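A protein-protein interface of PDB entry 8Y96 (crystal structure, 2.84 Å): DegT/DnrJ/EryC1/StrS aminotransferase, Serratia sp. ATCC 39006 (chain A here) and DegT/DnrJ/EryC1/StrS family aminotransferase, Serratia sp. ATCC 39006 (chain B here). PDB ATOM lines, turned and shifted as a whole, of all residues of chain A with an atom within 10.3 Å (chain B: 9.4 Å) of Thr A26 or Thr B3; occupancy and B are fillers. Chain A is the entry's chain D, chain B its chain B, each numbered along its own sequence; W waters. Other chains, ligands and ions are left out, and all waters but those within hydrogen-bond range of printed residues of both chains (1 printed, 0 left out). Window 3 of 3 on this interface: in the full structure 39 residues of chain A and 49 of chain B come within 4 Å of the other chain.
The side-chain hydroxyl of Thr B3 is in hydrogen-bond range of the backbone NH of Phe B5, 3.0 Å away. The backbone carbonyl oxygen of Ala A22 is in hydrogen-bond range of the side-chain hydroxyl of Thr A26 (2.6 Å). The side-chain hydroxyl of Ser A27 is in hydrogen-bond range of the backbone carbonyl oxygen of Val A24, 2.5 Å away. The side-chain hydroxyl of Ser A27 is in hydrogen-bond range of the backbone NH of Ile A29, at 2.9 Å.
CD1 of Ile B43 touches O of Leu A25, 3.5 Å away. CB of Leu A25 touches CD1 of Leu B48, 3.9 Å away. Leu A25 touches Met B51 (CD1 to CG, 3.9 Å). Leu A25 touches Phe B253. O of Lys B2 touches O of Thr A26 (3.6 Å). Thr B3 touches Thr A26 (CA to O, 3.5 Å). Asp B4 touches Thr A26 (N to O, 3.7 Å). CA of Ser A27 touches O of Lys B2, at 3.4 Å. Asp B4 touches Ser A27 (CB to O, 3.5 Å). Gly A28 touches Asp B4 (CA to OD2, 3.5 Å).
Thr B3 touches just one residue of chain A: Thr A26. Ser A27 touches two residues of chain B. No residue of chain A comes within 4 Å of Met B1. Printed residues of chain A within 4 Å of Pro B41: Ile A30. Printed residues of chain B within 4 Å of Leu A25: Ile B43 (3.5 Å), Leu B48 (3.9 Å), Met B51 (3.9 Å) and Phe B253 (3.7 Å). Of the printed residues of chain A, Ile B43 touches Leu A25. Lys B45 touches none of the printed residues of chain A. Arg A23 touches none of the printed residues of chain B. The nearest residue of chain A that does not touch Thr B3 is Ser A27 (4.3 Å).
Hydrophobic or aromatic side chains of chain B within 4 Å of the printed part of chain A: Pro B41, Ile B43, Leu B48, Met B51 and Phe B253. Printed residues of chain A that touch a printed residue of chain B: Leu A25, Thr A26, Ser A27, Gly A28 and Ile A30. Hydrophobic or aromatic side chains of chain A within 4 Å of the printed part of chain B: Leu A25 and Ile A30. Among the printed residues, 11 pairs touch across the chains. Among the printed residues, no Asp or Glu carboxylate lies within 4 Å of a Lys or Arg side-chain nitrogen of the other chain.
Water W1 bridges O of Lys B2 and O of Arg A23.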
ATOM      1  N   SER A  18     -17.227  31.254   6.634  1.00  0.00           N
ATOM      2  CA  SER A  18     -17.218  31.172   5.182  1.00  0.00           C
ATOM      3  C   SER A  18     -17.293  29.718   4.720  1.00  0.00           C
ATOM      4  O   SER A  18     -18.019  29.401   3.781  1.00  0.00           O
ATOM      5  CB  SER A  18     -16.001  31.866   4.617  1.00  0.00           C
ATOM      6  OG  SER A  18     -16.045  33.259   4.895  1.00  0.00           O
ATOM      7  N   PHE A  19     -16.535  28.842   5.389  1.00  0.00           N
ATOM      8  CA  PHE A  19     -16.408  27.451   4.989  1.00  0.00           C
ATOM      9  C   PHE A  19     -17.762  26.751   5.083  1.00  0.00           C
ATOM     10  O   PHE A  19     -18.110  25.954   4.215  1.00  0.00           O
ATOM     11  CB  PHE A  19     -15.357  26.736   5.847  1.00  0.00           C
ATOM     12  CG  PHE A  19     -15.143  25.291   5.423  1.00  0.00           C
ATOM     13  CD1 PHE A  19     -15.963  24.276   5.912  1.00  0.00           C
ATOM     14  CD2 PHE A  19     -14.151  24.960   4.508  1.00  0.00           C
ATOM     15  CE1 PHE A  19     -15.787  22.964   5.499  1.00  0.00           C
ATOM     16  CE2 PHE A  19     -13.977  23.646   4.095  1.00  0.00           C
ATOM     17  CZ  PHE A  19     -14.793  22.651   4.593  1.00  0.00           C
ATOM     18  N   VAL A  20     -18.510  27.043   6.149  1.00  0.00           N
ATOM     19  CA  VAL A  20     -19.777  26.374   6.399  1.00  0.00           C
ATOM     20  C   VAL A  20     -20.812  26.896   5.405  1.00  0.00           C
ATOM     21  O   VAL A  20     -21.548  26.114   4.810  1.00  0.00           O
ATOM     22  CB  VAL A  20     -20.218  26.526   7.871  1.00  0.00           C
ATOM     23  CG1 VAL A  20     -21.731  26.476   8.057  1.00  0.00           C
ATOM     24  CG2 VAL A  20     -19.545  25.479   8.754  1.00  0.00           C
ATOM     25  N   LEU A  21     -20.839  28.217   5.212  1.00  0.00           N
ATOM     26  CA  LEU A  21     -21.750  28.830   4.263  1.00  0.00           C
ATOM     27  C   LEU A  21     -21.447  28.311   2.860  1.00  0.00           C
ATOM     28  O   LEU A  21     -22.363  28.002   2.096  1.00  0.00           O
ATOM     29  CB  LEU A  21     -21.642  30.349   4.361  1.00  0.00           C
ATOM     30  CG  LEU A  21     -22.161  30.960   5.667  1.00  0.00           C
ATOM     31  CD1 LEU A  21     -21.732  32.407   5.799  1.00  0.00           C
ATOM     32  CD2 LEU A  21     -23.675  30.849   5.765  1.00  0.00           C
ATOM     33  N   ALA A  22     -20.154  28.191   2.538  1.00  0.00           N
ATOM     34  CA  ALA A  22     -19.735  27.578   1.288  1.00  0.00           C
ATOM     35  C   ALA A  22     -20.289  26.156   1.202  1.00  0.00           C
ATOM     36  O   ALA A  22     -20.905  25.796   0.200  1.00  0.00           O
ATOM     37  CB  ALA A  22     -18.225  27.603   1.168  1.00  0.00           C
ATOM     38  N   ARG A  23     -20.090  25.370   2.273  1.00  0.00           N
ATOM     39  CA  ARG A  23     -20.414  23.951   2.274  1.00  0.00           C
ATOM     40  C   ARG A  23     -21.899  23.743   1.991  1.00  0.00           C
ATOM     41  O   ARG A  23     -22.258  22.924   1.143  1.00  0.00           O
ATOM     42  CB  ARG A  23     -20.072  23.260   3.601  1.00  0.00           C
ATOM     43  CG  ARG A  23     -20.358  21.763   3.597  1.00  0.00           C
ATOM     44  CD  ARG A  23     -19.917  21.051   4.865  1.00  0.00           C
ATOM     45  NE  ARG A  23     -20.530  21.625   6.069  1.00  0.00           N
ATOM     46  CZ  ARG A  23     -21.826  21.626   6.379  1.00  0.00           C
ATOM     47  NH1 ARG A  23     -22.698  20.955   5.653  1.00  0.00           N
ATOM     48  NH2 ARG A  23     -22.248  22.292   7.438  1.00  0.00           N
ATOM     49  N   VAL A  24     -22.743  24.482   2.719  1.00  0.00           N
ATOM     50  CA  VAL A  24     -24.185  24.317   2.625  1.00  0.00           C
ATOM     51  C   VAL A  24     -24.663  24.809   1.258  1.00  0.00           C
ATOM     52  O   VAL A  24     -25.474  24.145   0.614  1.00  0.00           O
ATOM     53  CB  VAL A  24     -24.909  25.028   3.784  1.00  0.00           C
ATOM     54  CG1 VAL A  24     -26.425  24.946   3.652  1.00  0.00           C
ATOM     55  CG2 VAL A  24     -24.476  24.478   5.139  1.00  0.00           C
ATOM     56  N   LEU A  25     -24.141  25.959   0.807  1.00  0.00           N
ATOM     57  CA  LEU A  25     -24.470  26.486  -0.510  1.00  0.00           C
ATOM     58  C   LEU A  25     -24.120  25.457  -1.585  1.00  0.00           C
ATOM     59  O   LEU A  25     -24.864  25.284  -2.550  1.00  0.00           O
ATOM     60  CB  LEU A  25     -23.758  27.813  -0.774  1.00  0.00           C
ATOM     61  CG  LEU A  25     -24.314  29.047  -0.058  1.00  0.00           C
ATOM     62  CD1 LEU A  25     -23.359  30.211  -0.239  1.00  0.00           C
ATOM     63  CD2 LEU A  25     -25.702  29.423  -0.540  1.00  0.00           C
ATOM     64  N   THR A  26     -22.978  24.778  -1.416  1.00  0.00           N
ATOM     65  CA  THR A  26     -22.536  23.794  -2.390  1.00  0.00           C
ATOM     66  C   THR A  26     -23.489  22.599  -2.373  1.00  0.00           C
ATOM     67  O   THR A  26     -23.715  21.986  -3.411  1.00  0.00           O
ATOM     68  CB  THR A  26     -21.088  23.397  -2.113  1.00  0.00           C
ATOM     69  OG1 THR A  26     -20.376  24.630  -2.045  1.00  0.00           O
ATOM     70  CG2 THR A  26     -20.505  22.525  -3.209  1.00  0.00           C
ATOM     71  N   SER A  27     -24.062  22.287  -1.202  1.00  0.00           N
ATOM     72  CA  SER A  27     -25.029  21.205  -1.083  1.00  0.00           C
ATOM     73  C   SER A  27     -26.269  21.498  -1.925  1.00  0.00           C
ATOM     74  O   SER A  27     -26.904  20.576  -2.434  1.00  0.00           O
ATOM     75  CB  SER A  27     -25.426  20.963   0.349  1.00  0.00           C
ATOM     76  OG  SER A  27     -26.495  21.815   0.737  1.00  0.00           O
ATOM     77  N   GLY A  28     -26.623  22.784  -2.029  1.00  0.00           N
ATOM     78  CA  GLY A  28     -27.799  23.202  -2.771  1.00  0.00           C
ATOM     79  C   GLY A  28     -29.066  23.123  -1.921  1.00  0.00           C
ATOM     80  O   GLY A  28     -30.152  23.416  -2.417  1.00  0.00           O
ATOM     81  N   ILE A  29     -28.907  22.748  -0.641  1.00  0.00           N
ATOM     82  CA  ILE A  29     -30.021  22.545   0.274  1.00  0.00           C
ATOM     83  C   ILE A  29     -30.035  23.690   1.284  1.00  0.00           C
ATOM     84  O   ILE A  29     -29.319  23.640   2.283  1.00  0.00           O
ATOM     85  CB  ILE A  29     -29.908  21.184   0.992  1.00  0.00           C
ATOM     86  CG1 ILE A  29     -29.403  20.060   0.073  1.00  0.00           C
ATOM     87  CG2 ILE A  29     -31.232  20.818   1.669  1.00  0.00           C
ATOM     88  CD1 ILE A  29     -30.278  19.800  -1.140  1.00  0.00           C
ATOM     89  N   ILE A  30     -30.851  24.721   1.029  1.00  0.00           N
ATOM     90  CA  ILE A  30     -30.815  25.912   1.864  1.00  0.00           C
ATOM     91  C   ILE A  30     -32.212  26.285   2.350  1.00  0.00           C
ATOM     92  O   ILE A  30     -32.401  27.395   2.838  1.00  0.00           O
ATOM     93  CB  ILE A  30     -30.144  27.082   1.119  1.00  0.00           C
ATOM     94  CG1 ILE A  30     -30.930  27.507  -0.118  1.00  0.00           C
ATOM     95  CG2 ILE A  30     -28.696  26.742   0.768  1.00  0.00           C
ATOM     96  CD1 ILE A  30     -30.522  28.862  -0.665  1.00  0.00           C
ATOM     97  N   GLU A  34     -37.162  21.694   3.039  1.00  0.00           N
ATOM     98  CA  GLU A  34     -36.680  20.782   2.014  1.00  0.00           C
ATOM     99  C   GLU A  34     -36.293  19.452   2.657  1.00  0.00           C
ATOM    100  O   GLU A  34     -35.779  19.427   3.773  1.00  0.00           O
ATOM    101  CB  GLU A  34     -35.505  21.456   1.311  1.00  0.00           C
ATOM    102  CG  GLU A  34     -35.096  20.806  -0.007  1.00  0.00           C
ATOM    103  CD  GLU A  34     -34.035  21.610  -0.737  1.00  0.00           C
ATOM    104  OE1 GLU A  34     -33.706  22.724  -0.269  1.00  0.00           O
ATOM    105  OE2 GLU A  34     -33.529  21.119  -1.766  1.00  0.00           O
ATOM    106  N   ASN A  36     -33.982  16.143   3.110  1.00  0.00           N
ATOM    107  CA  ASN A  36     -32.532  16.005   3.151  1.00  0.00           C
ATOM    108  C   ASN A  36     -31.891  17.267   3.730  1.00  0.00           C
ATOM    109  O   ASN A  36     -30.843  17.692   3.252  1.00  0.00           O
ATOM    110  CB  ASN A  36     -31.902  15.735   1.783  1.00  0.00           C
ATOM    111  CG  ASN A  36     -32.620  14.676   0.979  1.00  0.00           C
ATOM    112  OD1 ASN A  36     -32.720  13.521   1.411  1.00  0.00           O
ATOM    113  ND2 ASN A  36     -33.106  15.041  -0.200  1.00  0.00           N
ATOM    114  N   GLU A  39     -29.103  20.296   8.768  1.00  0.00           N
ATOM    115  CA  GLU A  39     -28.351  21.300   9.502  1.00  0.00           C
ATOM    116  C   GLU A  39     -29.110  21.686  10.769  1.00  0.00           C
ATOM    117  O   GLU A  39     -28.507  21.810  11.830  1.00  0.00           O
ATOM    118  CB  GLU A  39     -28.026  22.506   8.618  1.00  0.00           C
ATOM    119  CG  GLU A  39     -27.229  22.142   7.367  1.00  0.00           C
ATOM    120  CD  GLU A  39     -25.827  21.608   7.620  1.00  0.00           C
ATOM    121  OE1 GLU A  39     -25.308  21.784   8.743  1.00  0.00           O
ATOM    122  OE2 GLU A  39     -25.256  20.998   6.692  1.00  0.00           O
ATOM    123  N   LEU A 196     -28.914  27.855   6.474  1.00  0.00           N
ATOM    124  CA  LEU A 196     -27.638  28.551   6.401  1.00  0.00           C
ATOM    125  C   LEU A 196     -27.278  29.111   7.774  1.00  0.00           C
ATOM    126  O   LEU A 196     -26.154  28.930   8.231  1.00  0.00           O
ATOM    127  CB  LEU A 196     -27.667  29.652   5.343  1.00  0.00           C
ATOM    128  CG  LEU A 196     -27.474  29.205   3.890  1.00  0.00           C
ATOM    129  CD1 LEU A 196     -27.761  30.361   2.957  1.00  0.00           C
ATOM    130  CD2 LEU A 196     -26.074  28.666   3.639  1.00  0.00           C
ATOM    131  N   MET B   1     -17.424  15.810  -0.939  1.00  0.00           N
ATOM    132  CA  MET B   1     -18.153  17.070  -1.241  1.00  0.00           C
ATOM    133  C   MET B   1     -19.570  16.735  -1.697  1.00  0.00           C
ATOM    134  O   MET B   1     -19.759  16.198  -2.786  1.00  0.00           O
ATOM    135  CB  MET B   1     -17.438  17.870  -2.336  1.00  0.00           C
ATOM    136  CG  MET B   1     -18.161  19.140  -2.743  1.00  0.00           C
ATOM    137  SD  MET B   1     -17.200  20.159  -3.878  1.00  0.00           S
ATOM    138  CE  MET B   1     -17.293  19.150  -5.364  1.00  0.00           C
ATOM    139  N   LYS B   2     -20.554  17.058  -0.848  1.00  0.00           N
ATOM    140  CA  LYS B   2     -21.950  16.885  -1.204  1.00  0.00           C
ATOM    141  C   LYS B   2     -22.348  18.041  -2.118  1.00  0.00           C
ATOM    142  O   LYS B   2     -22.307  19.197  -1.699  1.00  0.00           O
ATOM    143  CB  LYS B   2     -22.851  16.836   0.038  1.00  0.00           C
ATOM    144  CG  LYS B   2     -24.151  16.052  -0.148  1.00  0.00           C
ATOM    145  CD  LYS B   2     -25.421  16.769   0.302  1.00  0.00           C
ATOM    146  CE  LYS B   2     -25.472  17.139   1.752  1.00  0.00           C
ATOM    147  NZ  LYS B   2     -25.732  15.981   2.608  1.00  0.00           N
ATOM    148  N   THR B   3     -22.716  17.715  -3.366  1.00  0.00           N
ATOM    149  CA  THR B   3     -23.075  18.712  -4.363  1.00  0.00           C
ATOM    150  C   THR B   3     -24.395  18.318  -5.024  1.00  0.00           C
ATOM    151  O   THR B   3     -24.731  17.137  -5.098  1.00  0.00           O
ATOM    152  CB  THR B   3     -21.953  18.857  -5.393  1.00  0.00           C
ATOM    153  OG1 THR B   3     -22.513  19.625  -6.453  1.00  0.00           O
ATOM    154  CG2 THR B   3     -21.461  17.532  -5.948  1.00  0.00           C
ATOM    155  N   ASP B   4     -25.125  19.327  -5.521  1.00  0.00           N
ATOM    156  CA  ASP B   4     -26.381  19.110  -6.221  1.00  0.00           C
ATOM    157  C   ASP B   4     -26.141  19.020  -7.729  1.00  0.00           C
ATOM    158  O   ASP B   4     -27.074  18.754  -8.483  1.00  0.00           O
ATOM    159  CB  ASP B   4     -27.407  20.179  -5.873  1.00  0.00           C
ATOM    160  CG  ASP B   4     -27.049  21.605  -6.268  1.00  0.00           C
ATOM    161  OD1 ASP B   4     -25.889  21.838  -6.674  1.00  0.00           O
ATOM    162  OD2 ASP B   4     -27.936  22.474  -6.174  1.00  0.00           O
ATOM    163  N   PHE B   5     -24.891  19.234  -8.165  1.00  0.00           N
ATOM    164  CA  PHE B   5     -24.562  19.285  -9.582  1.00  0.00           C
ATOM    165  C   PHE B   5     -25.164  18.081 -10.302  1.00  0.00           C
ATOM    166  O   PHE B   5     -24.899  16.936  -9.936  1.00  0.00           O
ATOM    167  CB  PHE B   5     -23.048  19.326  -9.807  1.00  0.00           C
ATOM    168  CG  PHE B   5     -22.665  19.688 -11.236  1.00  0.00           C
ATOM    169  CD1 PHE B   5     -22.678  21.013 -11.657  1.00  0.00           C
ATOM    170  CD2 PHE B   5     -22.309  18.709 -12.156  1.00  0.00           C
ATOM    171  CE1 PHE B   5     -22.339  21.349 -12.958  1.00  0.00           C
ATOM    172  CE2 PHE B   5     -21.971  19.052 -13.458  1.00  0.00           C
ATOM    173  CZ  PHE B   5     -21.987  20.370 -13.855  1.00  0.00           C
ATOM    174  N   ILE B   6     -25.983  18.365 -11.323  1.00  0.00           N
ATOM    175  CA  ILE B   6     -26.557  17.341 -12.183  1.00  0.00           C
ATOM    176  C   ILE B   6     -25.489  16.915 -13.190  1.00  0.00           C
ATOM    177  O   ILE B   6     -24.924  17.760 -13.878  1.00  0.00           O
ATOM    178  CB  ILE B   6     -27.841  17.867 -12.856  1.00  0.00           C
ATOM    179  CG1 ILE B   6     -28.918  18.183 -11.808  1.00  0.00           C
ATOM    180  CG2 ILE B   6     -28.358  16.892 -13.915  1.00  0.00           C
ATOM    181  CD1 ILE B   6     -30.079  19.017 -12.323  1.00  0.00           C
ATOM    182  N   MET B   7     -25.224  15.602 -13.260  1.00  0.00           N
ATOM    183  CA  MET B   7     -24.079  15.065 -13.985  1.00  0.00           C
ATOM    184  C   MET B   7     -24.455  14.625 -15.399  1.00  0.00           C
ATOM    185  O   MET B   7     -23.574  14.457 -16.238  1.00  0.00           O
ATOM    186  CB  MET B   7     -23.480  13.856 -13.255  1.00  0.00           C
ATOM    187  CG  MET B   7     -22.632  14.202 -12.042  1.00  0.00           C
ATOM    188  SD  MET B   7     -21.222  15.266 -12.407  1.00  0.00           S
ATOM    189  CE  MET B   7     -20.473  14.488 -13.847  1.00  0.00           C
ATOM    190  N   ILE B  39     -32.513  22.257 -10.754  1.00  0.00           N
ATOM    191  CA  ILE B  39     -31.735  22.928  -9.720  1.00  0.00           C
ATOM    192  C   ILE B  39     -32.417  24.241  -9.354  1.00  0.00           C
ATOM    193  O   ILE B  39     -32.695  25.064 -10.227  1.00  0.00           O
ATOM    194  CB  ILE B  39     -30.286  23.157 -10.195  1.00  0.00           C
ATOM    195  CG1 ILE B  39     -29.475  21.862 -10.154  1.00  0.00           C
ATOM    196  CG2 ILE B  39     -29.599  24.275  -9.406  1.00  0.00           C
ATOM    197  CD1 ILE B  39     -29.509  21.144  -8.817  1.00  0.00           C
ATOM    198  N   PRO B  41     -32.229  27.042  -5.675  1.00  0.00           N
ATOM    199  CA  PRO B  41     -31.931  28.177  -6.552  1.00  0.00           C
ATOM    200  C   PRO B  41     -30.679  27.962  -7.393  1.00  0.00           C
ATOM    201  O   PRO B  41     -29.993  26.952  -7.253  1.00  0.00           O
ATOM    202  CB  PRO B  41     -31.761  29.352  -5.571  1.00  0.00           C
ATOM    203  CG  PRO B  41     -32.147  28.802  -4.212  1.00  0.00           C
ATOM    204  CD  PRO B  41     -31.844  27.318  -4.286  1.00  0.00           C
ATOM    205  N   ILE B  43     -27.393  28.561  -7.520  1.00  0.00           N
ATOM    206  CA  ILE B  43     -26.292  28.970  -6.669  1.00  0.00           C
ATOM    207  C   ILE B  43     -25.013  28.944  -7.500  1.00  0.00           C
ATOM    208  O   ILE B  43     -24.564  27.880  -7.918  1.00  0.00           O
ATOM    209  CB  ILE B  43     -26.208  28.088  -5.410  1.00  0.00           C
ATOM    210  CG1 ILE B  43     -27.498  28.202  -4.593  1.00  0.00           C
ATOM    211  CG2 ILE B  43     -24.976  28.442  -4.574  1.00  0.00           C
ATOM    212  CD1 ILE B  43     -27.504  27.421  -3.293  1.00  0.00           C
ATOM    213  N   ALA B  44     -24.453  30.136  -7.736  1.00  0.00           N
ATOM    214  CA  ALA B  44     -23.255  30.300  -8.544  1.00  0.00           C
ATOM    215  C   ALA B  44     -22.115  30.800  -7.665  1.00  0.00           C
ATOM    216  O   ALA B  44     -22.343  31.227  -6.536  1.00  0.00           O
ATOM    217  CB  ALA B  44     -23.528  31.256  -9.680  1.00  0.00           C
ATOM    218  N   LYS B  45     -20.897  30.748  -8.216  1.00  0.00           N
ATOM    219  CA  LYS B  45     -19.690  31.185  -7.530  1.00  0.00           C
ATOM    220  C   LYS B  45     -19.884  32.574  -6.924  1.00  0.00           C
ATOM    221  O   LYS B  45     -19.416  32.841  -5.819  1.00  0.00           O
ATOM    222  CB  LYS B  45     -18.497  31.181  -8.491  1.00  0.00           C
ATOM    223  CG  LYS B  45     -18.629  32.011  -9.769  1.00  0.00           C
ATOM    224  CD  LYS B  45     -17.465  31.763 -10.722  1.00  0.00           C
ATOM    225  CE  LYS B  45     -17.688  32.264 -12.109  1.00  0.00           C
ATOM    226  NZ  LYS B  45     -17.550  33.717 -12.210  1.00  0.00           N
ATOM    227  N   ASP B  47     -22.366  33.876  -5.548  1.00  0.00           N
ATOM    228  CA  ASP B  47     -23.106  33.839  -4.298  1.00  0.00           C
ATOM    229  C   ASP B  47     -22.180  33.442  -3.146  1.00  0.00           C
ATOM    230  O   ASP B  47     -22.334  33.949  -2.036  1.00  0.00           O
ATOM    231  CB  ASP B  47     -24.312  32.921  -4.405  1.00  0.00           C
ATOM    232  CG  ASP B  47     -25.248  33.192  -5.574  1.00  0.00           C
ATOM    233  OD1 ASP B  47     -25.674  34.357  -5.743  1.00  0.00           O
ATOM    234  OD2 ASP B  47     -25.553  32.230  -6.306  1.00  0.00           O
ATOM    235  N   LEU B  48     -21.238  32.526  -3.419  1.00  0.00           N
ATOM    236  CA  LEU B  48     -20.251  32.102  -2.437  1.00  0.00           C
ATOM    237  C   LEU B  48     -19.304  33.258  -2.133  1.00  0.00           C
ATOM    238  O   LEU B  48     -18.938  33.479  -0.982  1.00  0.00           O
ATOM    239  CB  LEU B  48     -19.457  30.889  -2.920  1.00  0.00           C
ATOM    240  CG  LEU B  48     -20.075  29.517  -2.643  1.00  0.00           C
ATOM    241  CD1 LEU B  48     -21.334  29.291  -3.463  1.00  0.00           C
ATOM    242  CD2 LEU B  48     -19.050  28.429  -2.912  1.00  0.00           C
ATOM    243  N   MET B  51     -20.771  35.951   0.024  1.00  0.00           N
ATOM    244  CA  MET B  51     -20.826  35.609   1.436  1.00  0.00           C
ATOM    245  C   MET B  51     -19.512  35.976   2.117  1.00  0.00           C
ATOM    246  O   MET B  51     -19.508  36.297   3.303  1.00  0.00           O
ATOM    247  CB  MET B  51     -21.108  34.118   1.645  1.00  0.00           C
ATOM    248  CG  MET B  51     -22.522  33.718   1.306  1.00  0.00           C
ATOM    249  SD  MET B  51     -23.728  34.460   2.423  1.00  0.00           S
ATOM    250  CE  MET B  51     -25.183  33.836   1.574  1.00  0.00           C
ATOM    251  N   PHE B 253     -27.184  36.618   0.200  1.00  0.00           N
ATOM    252  CA  PHE B 253     -27.566  35.793  -0.933  1.00  0.00           C
ATOM    253  C   PHE B 253     -28.433  36.615  -1.888  1.00  0.00           C
ATOM    254  O   PHE B 253     -28.298  36.498  -3.103  1.00  0.00           O
ATOM    255  CB  PHE B 253     -28.251  34.529  -0.404  1.00  0.00           C
ATOM    256  CG  PHE B 253     -28.454  33.447  -1.455  1.00  0.00           C
ATOM    257  CD1 PHE B 253     -27.392  32.652  -1.870  1.00  0.00           C
ATOM    258  CD2 PHE B 253     -29.702  33.232  -2.027  1.00  0.00           C
ATOM    259  CE1 PHE B 253     -27.575  31.675  -2.833  1.00  0.00           C
ATOM    260  CE2 PHE B 253     -29.881  32.254  -2.989  1.00  0.00           C
ATOM    261  CZ  PHE B 253     -28.818  31.477  -3.388  1.00  0.00           C
HETATM  262  O   HOH W   1     -21.534  20.361   0.496  1.00  0.00           O
